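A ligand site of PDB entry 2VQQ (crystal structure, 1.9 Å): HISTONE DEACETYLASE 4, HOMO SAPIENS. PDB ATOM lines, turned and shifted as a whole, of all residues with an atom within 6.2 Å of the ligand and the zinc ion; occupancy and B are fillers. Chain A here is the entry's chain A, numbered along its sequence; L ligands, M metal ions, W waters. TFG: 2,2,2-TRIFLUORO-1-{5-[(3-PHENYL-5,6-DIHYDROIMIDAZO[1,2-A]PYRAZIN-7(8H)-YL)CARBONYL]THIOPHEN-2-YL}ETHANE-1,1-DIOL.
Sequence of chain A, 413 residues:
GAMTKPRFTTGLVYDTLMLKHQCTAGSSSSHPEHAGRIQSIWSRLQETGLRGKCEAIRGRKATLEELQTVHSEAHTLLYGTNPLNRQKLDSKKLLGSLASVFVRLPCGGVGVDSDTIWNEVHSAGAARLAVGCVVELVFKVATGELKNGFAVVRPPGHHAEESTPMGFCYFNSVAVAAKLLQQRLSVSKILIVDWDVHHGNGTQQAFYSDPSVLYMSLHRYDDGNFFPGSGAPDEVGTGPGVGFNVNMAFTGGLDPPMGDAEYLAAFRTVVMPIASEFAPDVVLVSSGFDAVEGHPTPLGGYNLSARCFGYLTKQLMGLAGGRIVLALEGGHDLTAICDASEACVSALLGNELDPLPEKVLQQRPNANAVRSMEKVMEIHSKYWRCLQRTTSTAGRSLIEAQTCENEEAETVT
OD1 of Asp 290 is in hydrogen-bond range of N of Val 197 (2.7 Å). The backbone carbonyl oxygen (O) of Leu 299 is in hydrogen-bond range of a ring nitrogen (NE2) of His 332 (3.2 Å). A ring nitrogen (ND1) of His 159 lies close to the backbone carbonyl oxygen (O) of His 199 (3.3 Å). OE1 of Glu 329 lies within hydrogen-bond range of N of Gly 157, at 2.9 Å. O of Pro 156 sits at hydrogen-bond distance from SG of Cys 169, at 3.2 Å. A ring nitrogen (NE2) of His 159 sits at hydrogen-bond distance from a ring nitrogen (NE2) of His 158 (3.3 Å). The backbone NH of Gly 157 is in hydrogen-bond range of the side-chain sulfur of Cys 169. The side-chain sulfur of Cys 169 sits at hydrogen-bond distance from the backbone NH of His 159 (3.5 Å).
F2 of the ligand sits close to O of Gly 167 (3.0 Å). The backbone NH (N) of Gly 330 sits close to a fluorine (F1) of the ligand (3.0 Å). Pro 156 touches the ligand. CD1 of Phe 168 touches C2 of the ligand (3.6 Å). Cys 169 touches the ligand (SG to F2, 3.8 Å). Phe 227 touches the ligand (CE2 to C3, 3.3 Å). Leu 299 touches the ligand. C of Glu 329 touches F1 of the ligand, 3.8 Å away. 13 residues have an atom within 4 Å of the ligand: Pro 156, His 158, His 159, Gly 167, Phe 168, Cys 169, Asp 196, His 198, Phe 227, Asp 290, Leu 299, Glu 329 and Gly 330. The nearest printed residue that does not touch the ligand is Gly 331 (4.4 Å).
An oxygen (O3) of the ligand sits close to a ring nitrogen (NE2) of His 158 (3.1 Å). A ring nitrogen (NE2) of His 159 lies close to an oxygen (O3) of the ligand (2.8 Å).
Water W1 lies within hydrogen-bond range of O of Pro 298 (2.6 Å), O1 of the ligand (2.7 Å) and NE2 of His 198 (3.4 Å).
The zinc ion is bound by the side-chain carboxylate (OD2) of Asp 290, an oxygen (O2) of the ligand, the side-chain carboxylate (OD2) of Asp 196, a ring nitrogen (ND1) of His 198 and an oxygen (O3) of the ligand.
Three residues have an atom within 4 Å of the zinc ion: Asp 196, His 198 and Asp 290. The nearest printed residue that does not touch the zinc ion is Val 197 (4.3 Å).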
ATOM      1  N   ARG A  37     -15.765  -5.890  12.076  1.00  0.00           N
ATOM      2  CA  ARG A  37     -15.781  -6.383  10.681  1.00  0.00           C
ATOM      3  C   ARG A  37     -15.039  -7.709  10.501  1.00  0.00           C
ATOM      4  O   ARG A  37     -15.645  -8.686  10.066  1.00  0.00           O
ATOM      5  CB  ARG A  37     -15.178  -5.327   9.745  1.00  0.00           C
ATOM      6  CG  ARG A  37     -16.019  -4.053   9.615  1.00  0.00           C
ATOM      7  CD  ARG A  37     -15.463  -3.118   8.532  1.00  0.00           C
ATOM      8  NE  ARG A  37     -14.010  -3.008   8.622  1.00  0.00           N
ATOM      9  CZ  ARG A  37     -13.145  -3.191   7.626  1.00  0.00           C
ATOM     10  NH1 ARG A  37     -13.531  -3.430   6.372  1.00  0.00           N
ATOM     11  NH2 ARG A  37     -11.857  -3.087   7.882  1.00  0.00           N
ATOM     12  N   PRO A 156      -7.504  -1.379   6.567  1.00  0.00           N
ATOM     13  CA  PRO A 156      -7.192  -1.418   5.134  1.00  0.00           C
ATOM     14  C   PRO A 156      -5.860  -0.719   4.836  1.00  0.00           C
ATOM     15  O   PRO A 156      -5.320  -0.015   5.695  1.00  0.00           O
ATOM     16  CB  PRO A 156      -8.372  -0.675   4.486  1.00  0.00           C
ATOM     17  CG  PRO A 156      -8.893   0.209   5.560  1.00  0.00           C
ATOM     18  CD  PRO A 156      -8.690  -0.535   6.838  1.00  0.00           C
ATOM     19  N   GLY A 157      -5.329  -0.936   3.636  1.00  0.00           N
ATOM     20  CA  GLY A 157      -4.026  -0.422   3.242  1.00  0.00           C
ATOM     21  C   GLY A 157      -3.948   0.470   2.017  1.00  0.00           C
ATOM     22  O   GLY A 157      -2.988   1.222   1.858  1.00  0.00           O
ATOM     23  N   HIS A 158      -4.945   0.386   1.135  1.00  0.00           N
ATOM     24  CA  HIS A 158      -4.787   0.899  -0.228  1.00  0.00           C
ATOM     25  C   HIS A 158      -4.699   2.427  -0.370  1.00  0.00           C
ATOM     26  O   HIS A 158      -4.265   2.915  -1.422  1.00  0.00           O
ATOM     27  CB  HIS A 158      -5.809   0.267  -1.189  1.00  0.00           C
ATOM     28  CG  HIS A 158      -7.221   0.795  -1.066  1.00  0.00           C
ATOM     29  ND1 HIS A 158      -8.075   0.848  -2.138  1.00  0.00           N
ATOM     30  CD2 HIS A 158      -7.916   1.272  -0.005  1.00  0.00           C
ATOM     31  CE1 HIS A 158      -9.242   1.340  -1.750  1.00  0.00           C
ATOM     32  NE2 HIS A 158      -9.171   1.606  -0.459  1.00  0.00           N
ATOM     33  N   HIS A 159      -5.053   3.191   0.673  1.00  0.00           N
ATOM     34  CA  HIS A 159      -4.880   4.658   0.629  1.00  0.00           C
ATOM     35  C   HIS A 159      -3.522   5.150   1.143  1.00  0.00           C
ATOM     36  O   HIS A 159      -3.142   6.286   0.861  1.00  0.00           O
ATOM     37  CB  HIS A 159      -5.998   5.388   1.397  1.00  0.00           C
ATOM     38  CG  HIS A 159      -7.371   5.174   0.831  1.00  0.00           C
ATOM     39  ND1 HIS A 159      -7.694   5.466  -0.477  1.00  0.00           N
ATOM     40  CD2 HIS A 159      -8.511   4.732   1.413  1.00  0.00           C
ATOM     41  CE1 HIS A 159      -8.972   5.191  -0.681  1.00  0.00           C
ATOM     42  NE2 HIS A 159      -9.493   4.738   0.441  1.00  0.00           N
ATOM     43  N   MET A 166      -3.569   7.804   5.562  1.00  0.00           N
ATOM     44  CA  MET A 166      -4.833   8.472   5.240  1.00  0.00           C
ATOM     45  C   MET A 166      -5.915   7.448   4.990  1.00  0.00           C
ATOM     46  O   MET A 166      -5.625   6.283   4.721  1.00  0.00           O
ATOM     47  CB  MET A 166      -4.697   9.379   4.019  1.00  0.00           C
ATOM     48  CG  MET A 166      -4.094   8.717   2.785  1.00  0.00           C
ATOM     49  SD  MET A 166      -3.999   9.845   1.361  1.00  0.00           S
ATOM     50  CE  MET A 166      -5.651   9.716   0.758  1.00  0.00           C
ATOM     51  N   GLY A 167      -7.167   7.890   5.077  1.00  0.00           N
ATOM     52  CA  GLY A 167      -8.319   7.024   4.823  1.00  0.00           C
ATOM     53  C   GLY A 167      -8.274   5.736   5.624  1.00  0.00           C
ATOM     54  O   GLY A 167      -8.513   4.661   5.079  1.00  0.00           O
ATOM     55  N   PHE A 168      -7.957   5.852   6.916  1.00  0.00           N
ATOM     56  CA  PHE A 168      -7.868   4.694   7.832  1.00  0.00           C
ATOM     57  C   PHE A 168      -6.675   3.743   7.570  1.00  0.00           C
ATOM     58  O   PHE A 168      -6.574   2.711   8.238  1.00  0.00           O
ATOM     59  CB  PHE A 168      -9.171   3.863   7.847  1.00  0.00           C
ATOM     60  CG  PHE A 168     -10.430   4.675   7.987  1.00  0.00           C
ATOM     61  CD1 PHE A 168     -11.392   4.657   6.998  1.00  0.00           C
ATOM     62  CD2 PHE A 168     -10.672   5.420   9.118  1.00  0.00           C
ATOM     63  CE1 PHE A 168     -12.576   5.386   7.118  1.00  0.00           C
ATOM     64  CE2 PHE A 168     -11.847   6.160   9.256  1.00  0.00           C
ATOM     65  CZ  PHE A 168     -12.796   6.138   8.246  1.00  0.00           C
ATOM     66  N   CYS A 169      -5.793   4.098   6.645  1.00  0.00           N
ATOM     67  CA  CYS A 169      -4.675   3.252   6.215  1.00  0.00           C
ATOM     68  C   CYS A 169      -3.332   3.796   6.701  1.00  0.00           C
ATOM     69  O   CYS A 169      -3.023   4.972   6.518  1.00  0.00           O
ATOM     70  CB  CYS A 169      -4.640   3.108   4.689  1.00  0.00           C
ATOM     71  SG  CYS A 169      -6.201   2.554   3.926  1.00  0.00           S
ATOM     72  N   ASP A 196     -12.544  -2.168  -4.281  1.00  0.00           N
ATOM     73  CA  ASP A 196     -13.077  -1.234  -3.287  1.00  0.00           C
ATOM     74  C   ASP A 196     -13.710  -0.069  -4.074  1.00  0.00           C
ATOM     75  O   ASP A 196     -13.215   0.306  -5.150  1.00  0.00           O
ATOM     76  CB  ASP A 196     -11.946  -0.767  -2.364  1.00  0.00           C
ATOM     77  CG  ASP A 196     -12.436   0.021  -1.152  1.00  0.00           C
ATOM     78  OD1 ASP A 196     -12.498  -0.538  -0.032  1.00  0.00           O
ATOM     79  OD2 ASP A 196     -12.792   1.196  -1.318  1.00  0.00           O
ATOM     80  N   VAL A 197     -14.789   0.499  -3.554  1.00  0.00           N
ATOM     81  CA  VAL A 197     -15.489   1.577  -4.269  1.00  0.00           C
ATOM     82  C   VAL A 197     -14.654   2.883  -4.351  1.00  0.00           C
ATOM     83  O   VAL A 197     -14.952   3.756  -5.168  1.00  0.00           O
ATOM     84  CB  VAL A 197     -16.900   1.830  -3.697  1.00  0.00           C
ATOM     85  CG1 VAL A 197     -16.864   2.739  -2.463  1.00  0.00           C
ATOM     86  CG2 VAL A 197     -17.843   2.418  -4.791  1.00  0.00           C
ATOM     87  N   HIS A 198     -13.617   3.015  -3.521  1.00  0.00           N
ATOM     88  CA  HIS A 198     -12.745   4.194  -3.551  1.00  0.00           C
ATOM     89  C   HIS A 198     -11.414   3.888  -4.250  1.00  0.00           C
ATOM     90  O   HIS A 198     -10.891   2.773  -4.148  1.00  0.00           O
ATOM     91  CB  HIS A 198     -12.486   4.708  -2.126  1.00  0.00           C
ATOM     92  CG  HIS A 198     -13.734   5.005  -1.359  1.00  0.00           C
ATOM     93  ND1 HIS A 198     -14.376   4.062  -0.584  1.00  0.00           N
ATOM     94  CD2 HIS A 198     -14.478   6.131  -1.284  1.00  0.00           C
ATOM     95  CE1 HIS A 198     -15.454   4.604  -0.049  1.00  0.00           C
ATOM     96  NE2 HIS A 198     -15.544   5.848  -0.471  1.00  0.00           N
ATOM     97  N   HIS A 199     -10.867   4.869  -4.974  1.00  0.00           N
ATOM     98  CA  HIS A 199      -9.607   4.705  -5.686  1.00  0.00           C
ATOM     99  C   HIS A 199      -8.445   4.364  -4.735  1.00  0.00           C
ATOM    100  O   HIS A 199      -8.255   5.017  -3.719  1.00  0.00           O
ATOM    101  CB  HIS A 199      -9.265   5.988  -6.442  1.00  0.00           C
ATOM    102  CG  HIS A 199      -7.994   5.914  -7.212  1.00  0.00           C
ATOM    103  ND1 HIS A 199      -6.914   6.736  -6.965  1.00  0.00           N
ATOM    104  CD2 HIS A 199      -7.611   5.098  -8.228  1.00  0.00           C
ATOM    105  CE1 HIS A 199      -5.931   6.434  -7.783  1.00  0.00           C
ATOM    106  NE2 HIS A 199      -6.327   5.443  -8.568  1.00  0.00           N
ATOM    107  N   PHE A 226     -15.231  12.557  -5.464  1.00  0.00           N
ATOM    108  CA  PHE A 226     -15.488  11.464  -4.536  1.00  0.00           C
ATOM    109  C   PHE A 226     -14.157  11.030  -3.895  1.00  0.00           C
ATOM    110  O   PHE A 226     -13.133  11.016  -4.567  1.00  0.00           O
ATOM    111  CB  PHE A 226     -16.152  10.305  -5.290  1.00  0.00           C
ATOM    112  CG  PHE A 226     -16.758   9.268  -4.398  1.00  0.00           C
ATOM    113  CD1 PHE A 226     -17.911   9.543  -3.674  1.00  0.00           C
ATOM    114  CD2 PHE A 226     -16.187   8.005  -4.281  1.00  0.00           C
ATOM    115  CE1 PHE A 226     -18.477   8.584  -2.831  1.00  0.00           C
ATOM    116  CE2 PHE A 226     -16.740   7.042  -3.458  1.00  0.00           C
ATOM    117  CZ  PHE A 226     -17.899   7.342  -2.719  1.00  0.00           C
ATOM    118  N   PHE A 227     -14.175  10.722  -2.591  1.00  0.00           N
ATOM    119  CA  PHE A 227     -12.936  10.392  -1.852  1.00  0.00           C
ATOM    120  C   PHE A 227     -12.178   9.238  -2.534  1.00  0.00           C
ATOM    121  O   PHE A 227     -12.793   8.244  -2.905  1.00  0.00           O
ATOM    122  CB  PHE A 227     -13.270  10.026  -0.392  1.00  0.00           C
ATOM    123  CG  PHE A 227     -12.044   9.737   0.453  1.00  0.00           C
ATOM    124  CD1 PHE A 227     -11.405  10.752   1.165  1.00  0.00           C
ATOM    125  CD2 PHE A 227     -11.525   8.446   0.538  1.00  0.00           C
ATOM    126  CE1 PHE A 227     -10.277  10.499   1.928  1.00  0.00           C
ATOM    127  CE2 PHE A 227     -10.396   8.178   1.304  1.00  0.00           C
ATOM    128  CZ  PHE A 227      -9.765   9.199   2.005  1.00  0.00           C
ATOM    129  N   GLY A 288     -12.178  -4.582  -1.259  1.00  0.00           N
ATOM    130  CA  GLY A 288     -13.116  -3.824  -0.459  1.00  0.00           C
ATOM    131  C   GLY A 288     -14.505  -4.186  -0.934  1.00  0.00           C
ATOM    132  O   GLY A 288     -14.704  -4.497  -2.116  1.00  0.00           O
ATOM    133  N   ASP A 290     -17.349  -2.109  -0.074  1.00  0.00           N
ATOM    134  CA  ASP A 290     -18.213  -0.921   0.099  1.00  0.00           C
ATOM    135  C   ASP A 290     -19.068  -0.562  -1.142  1.00  0.00           C
ATOM    136  O   ASP A 290     -19.899   0.333  -1.069  1.00  0.00           O
ATOM    137  CB  ASP A 290     -17.421   0.325   0.624  1.00  0.00           C
ATOM    138  CG  ASP A 290     -16.055   0.532  -0.032  1.00  0.00           C
ATOM    139  OD1 ASP A 290     -15.698  -0.139  -1.043  1.00  0.00           O
ATOM    140  OD2 ASP A 290     -15.308   1.406   0.504  1.00  0.00           O
ATOM    141  N   PRO A 298     -22.232   8.707   0.657  1.00  0.00           N
ATOM    142  CA  PRO A 298     -20.790   9.039   0.665  1.00  0.00           C
ATOM    143  C   PRO A 298     -19.821   7.870   0.970  1.00  0.00           C
ATOM    144  O   PRO A 298     -18.760   7.771   0.342  1.00  0.00           O
ATOM    145  CB  PRO A 298     -20.678  10.134   1.736  1.00  0.00           C
ATOM    146  CG  PRO A 298     -21.917  10.007   2.582  1.00  0.00           C
ATOM    147  CD  PRO A 298     -22.848   8.966   1.968  1.00  0.00           C
ATOM    148  N   LEU A 299     -20.189   6.995   1.906  1.00  0.00           N
ATOM    149  CA  LEU A 299     -19.373   5.835   2.261  1.00  0.00           C
ATOM    150  C   LEU A 299     -19.835   4.605   1.476  1.00  0.00           C
ATOM    151  O   LEU A 299     -20.004   3.515   2.031  1.00  0.00           O
ATOM    152  CB  LEU A 299     -19.491   5.549   3.762  1.00  0.00           C
ATOM    153  CG  LEU A 299     -19.159   6.685   4.738  1.00  0.00           C
ATOM    154  CD1 LEU A 299     -19.545   6.304   6.164  1.00  0.00           C
ATOM    155  CD2 LEU A 299     -17.681   7.039   4.638  1.00  0.00           C
ATOM    156  N   GLU A 329     -10.205  -4.809   2.183  1.00  0.00           N
ATOM    157  CA  GLU A 329      -9.937  -3.384   2.293  1.00  0.00           C
ATOM    158  C   GLU A 329     -11.128  -2.746   3.032  1.00  0.00           C
ATOM    159  O   GLU A 329     -11.325  -3.051   4.206  1.00  0.00           O
ATOM    160  CB  GLU A 329      -9.680  -2.772   0.915  1.00  0.00           C
ATOM    161  CG  GLU A 329      -8.431  -3.363   0.193  1.00  0.00           C
ATOM    162  CD  GLU A 329      -7.097  -2.760   0.647  1.00  0.00           C
ATOM    163  OE1 GLU A 329      -7.061  -1.917   1.567  1.00  0.00           O
ATOM    164  OE2 GLU A 329      -6.064  -3.154   0.057  1.00  0.00           O
ATOM    165  N   GLY A 330     -11.912  -1.905   2.358  1.00  0.00           N
ATOM    166  CA  GLY A 330     -13.083  -1.250   2.960  1.00  0.00           C
ATOM    167  C   GLY A 330     -14.373  -2.051   2.866  1.00  0.00           C
ATOM    168  O   GLY A 330     -14.365  -3.227   2.506  1.00  0.00           O
ATOM    169  N   GLY A 331     -15.480  -1.381   3.165  1.00  0.00           N
ATOM    170  CA  GLY A 331     -16.770  -2.010   3.447  1.00  0.00           C
ATOM    171  C   GLY A 331     -17.020  -1.973   4.947  1.00  0.00           C
ATOM    172  O   GLY A 331     -16.096  -2.103   5.722  1.00  0.00           O
ATOM    173  N   HIS A 332     -18.258  -1.762   5.372  1.00  0.00           N
ATOM    174  CA  HIS A 332     -18.562  -1.659   6.803  1.00  0.00           C
ATOM    175  C   HIS A 332     -19.911  -2.230   7.241  1.00  0.00           C
ATOM    176  O   HIS A 332     -20.061  -2.617   8.396  1.00  0.00           O
ATOM    177  CB  HIS A 332     -18.403  -0.201   7.281  1.00  0.00           C
ATOM    178  CG  HIS A 332     -19.092   0.799   6.417  1.00  0.00           C
ATOM    179  ND1 HIS A 332     -20.417   1.164   6.595  1.00  0.00           N
ATOM    180  CD2 HIS A 332     -18.642   1.530   5.359  1.00  0.00           C
ATOM    181  CE1 HIS A 332     -20.748   2.065   5.693  1.00  0.00           C
ATOM    182  NE2 HIS A 332     -19.693   2.300   4.931  1.00  0.00           N
HETATM  183  C14 TFG L   1     -17.561  12.464   7.756  1.00  0.00           C
HETATM  184  C15 TFG L   1     -18.754  13.195   7.733  1.00  0.00           C
HETATM  185  C16 TFG L   1     -19.736  12.864   6.805  1.00  0.00           C
HETATM  186  C17 TFG L   1     -19.510  11.830   5.892  1.00  0.00           C
HETATM  187  C18 TFG L   1     -18.315  11.102   5.935  1.00  0.00           C
HETATM  188  C13 TFG L   1     -17.333  11.407   6.879  1.00  0.00           C
HETATM  189  C19 TFG L   1     -16.102  10.718   6.932  1.00  0.00           C
HETATM  190  C12 TFG L   1     -15.352  10.355   7.967  1.00  0.00           C
HETATM  191  N3  TFG L   1     -14.239   9.748   7.544  1.00  0.00           N
HETATM  192  C11 TFG L   1     -14.233   9.711   6.204  1.00  0.00           C
HETATM  193  C10 TFG L   1     -13.180   9.132   5.208  1.00  0.00           C
HETATM  194  N2  TFG L   1     -15.433  10.333   5.794  1.00  0.00           N
HETATM  195  C9  TFG L   1     -15.833  10.492   4.395  1.00  0.00           C
HETATM  196  C8  TFG L   1     -14.709  10.180   3.476  1.00  0.00           C
HETATM  197  N1  TFG L   1     -13.900   9.025   3.933  1.00  0.00           N
HETATM  198  C7  TFG L   1     -14.005   7.930   3.168  1.00  0.00           C
HETATM  199  O1  TFG L   1     -14.692   8.044   2.144  1.00  0.00           O
HETATM  200  C4  TFG L   1     -13.223   6.648   3.253  1.00  0.00           C
HETATM  201  S1  TFG L   1     -13.760   5.250   2.535  1.00  0.00           S
HETATM  202  C3  TFG L   1     -11.956   6.493   3.661  1.00  0.00           C
HETATM  203  C2  TFG L   1     -11.462   5.244   3.474  1.00  0.00           C
HETATM  204  C1  TFG L   1     -12.328   4.407   2.837  1.00  0.00           C
HETATM  205  C5  TFG L   1     -12.115   2.961   2.412  1.00  0.00           C
HETATM  206  C6  TFG L   1     -11.176   2.099   3.273  1.00  0.00           C
HETATM  207  F1  TFG L   1     -11.028   0.984   2.586  1.00  0.00           F
HETATM  208  F2  TFG L   1      -9.982   2.672   3.458  1.00  0.00           F
HETATM  209  F3  TFG L   1     -11.728   1.807   4.449  1.00  0.00           F
HETATM  210  O3  TFG L   1     -11.529   2.951   1.046  1.00  0.00           O
HETATM  211  O2  TFG L   1     -13.386   2.328   2.254  1.00  0.00           O
HETATM  212 ZN    ZN M   1     -13.581   2.155   0.271  1.00  0.00          ZN
HETATM  213  O   HOH W   1     -16.439   8.976   0.338  1.00  0.00           O
HETATM  214  O   HOH W   2     -14.947   1.379   3.973  1.00  0.00           O
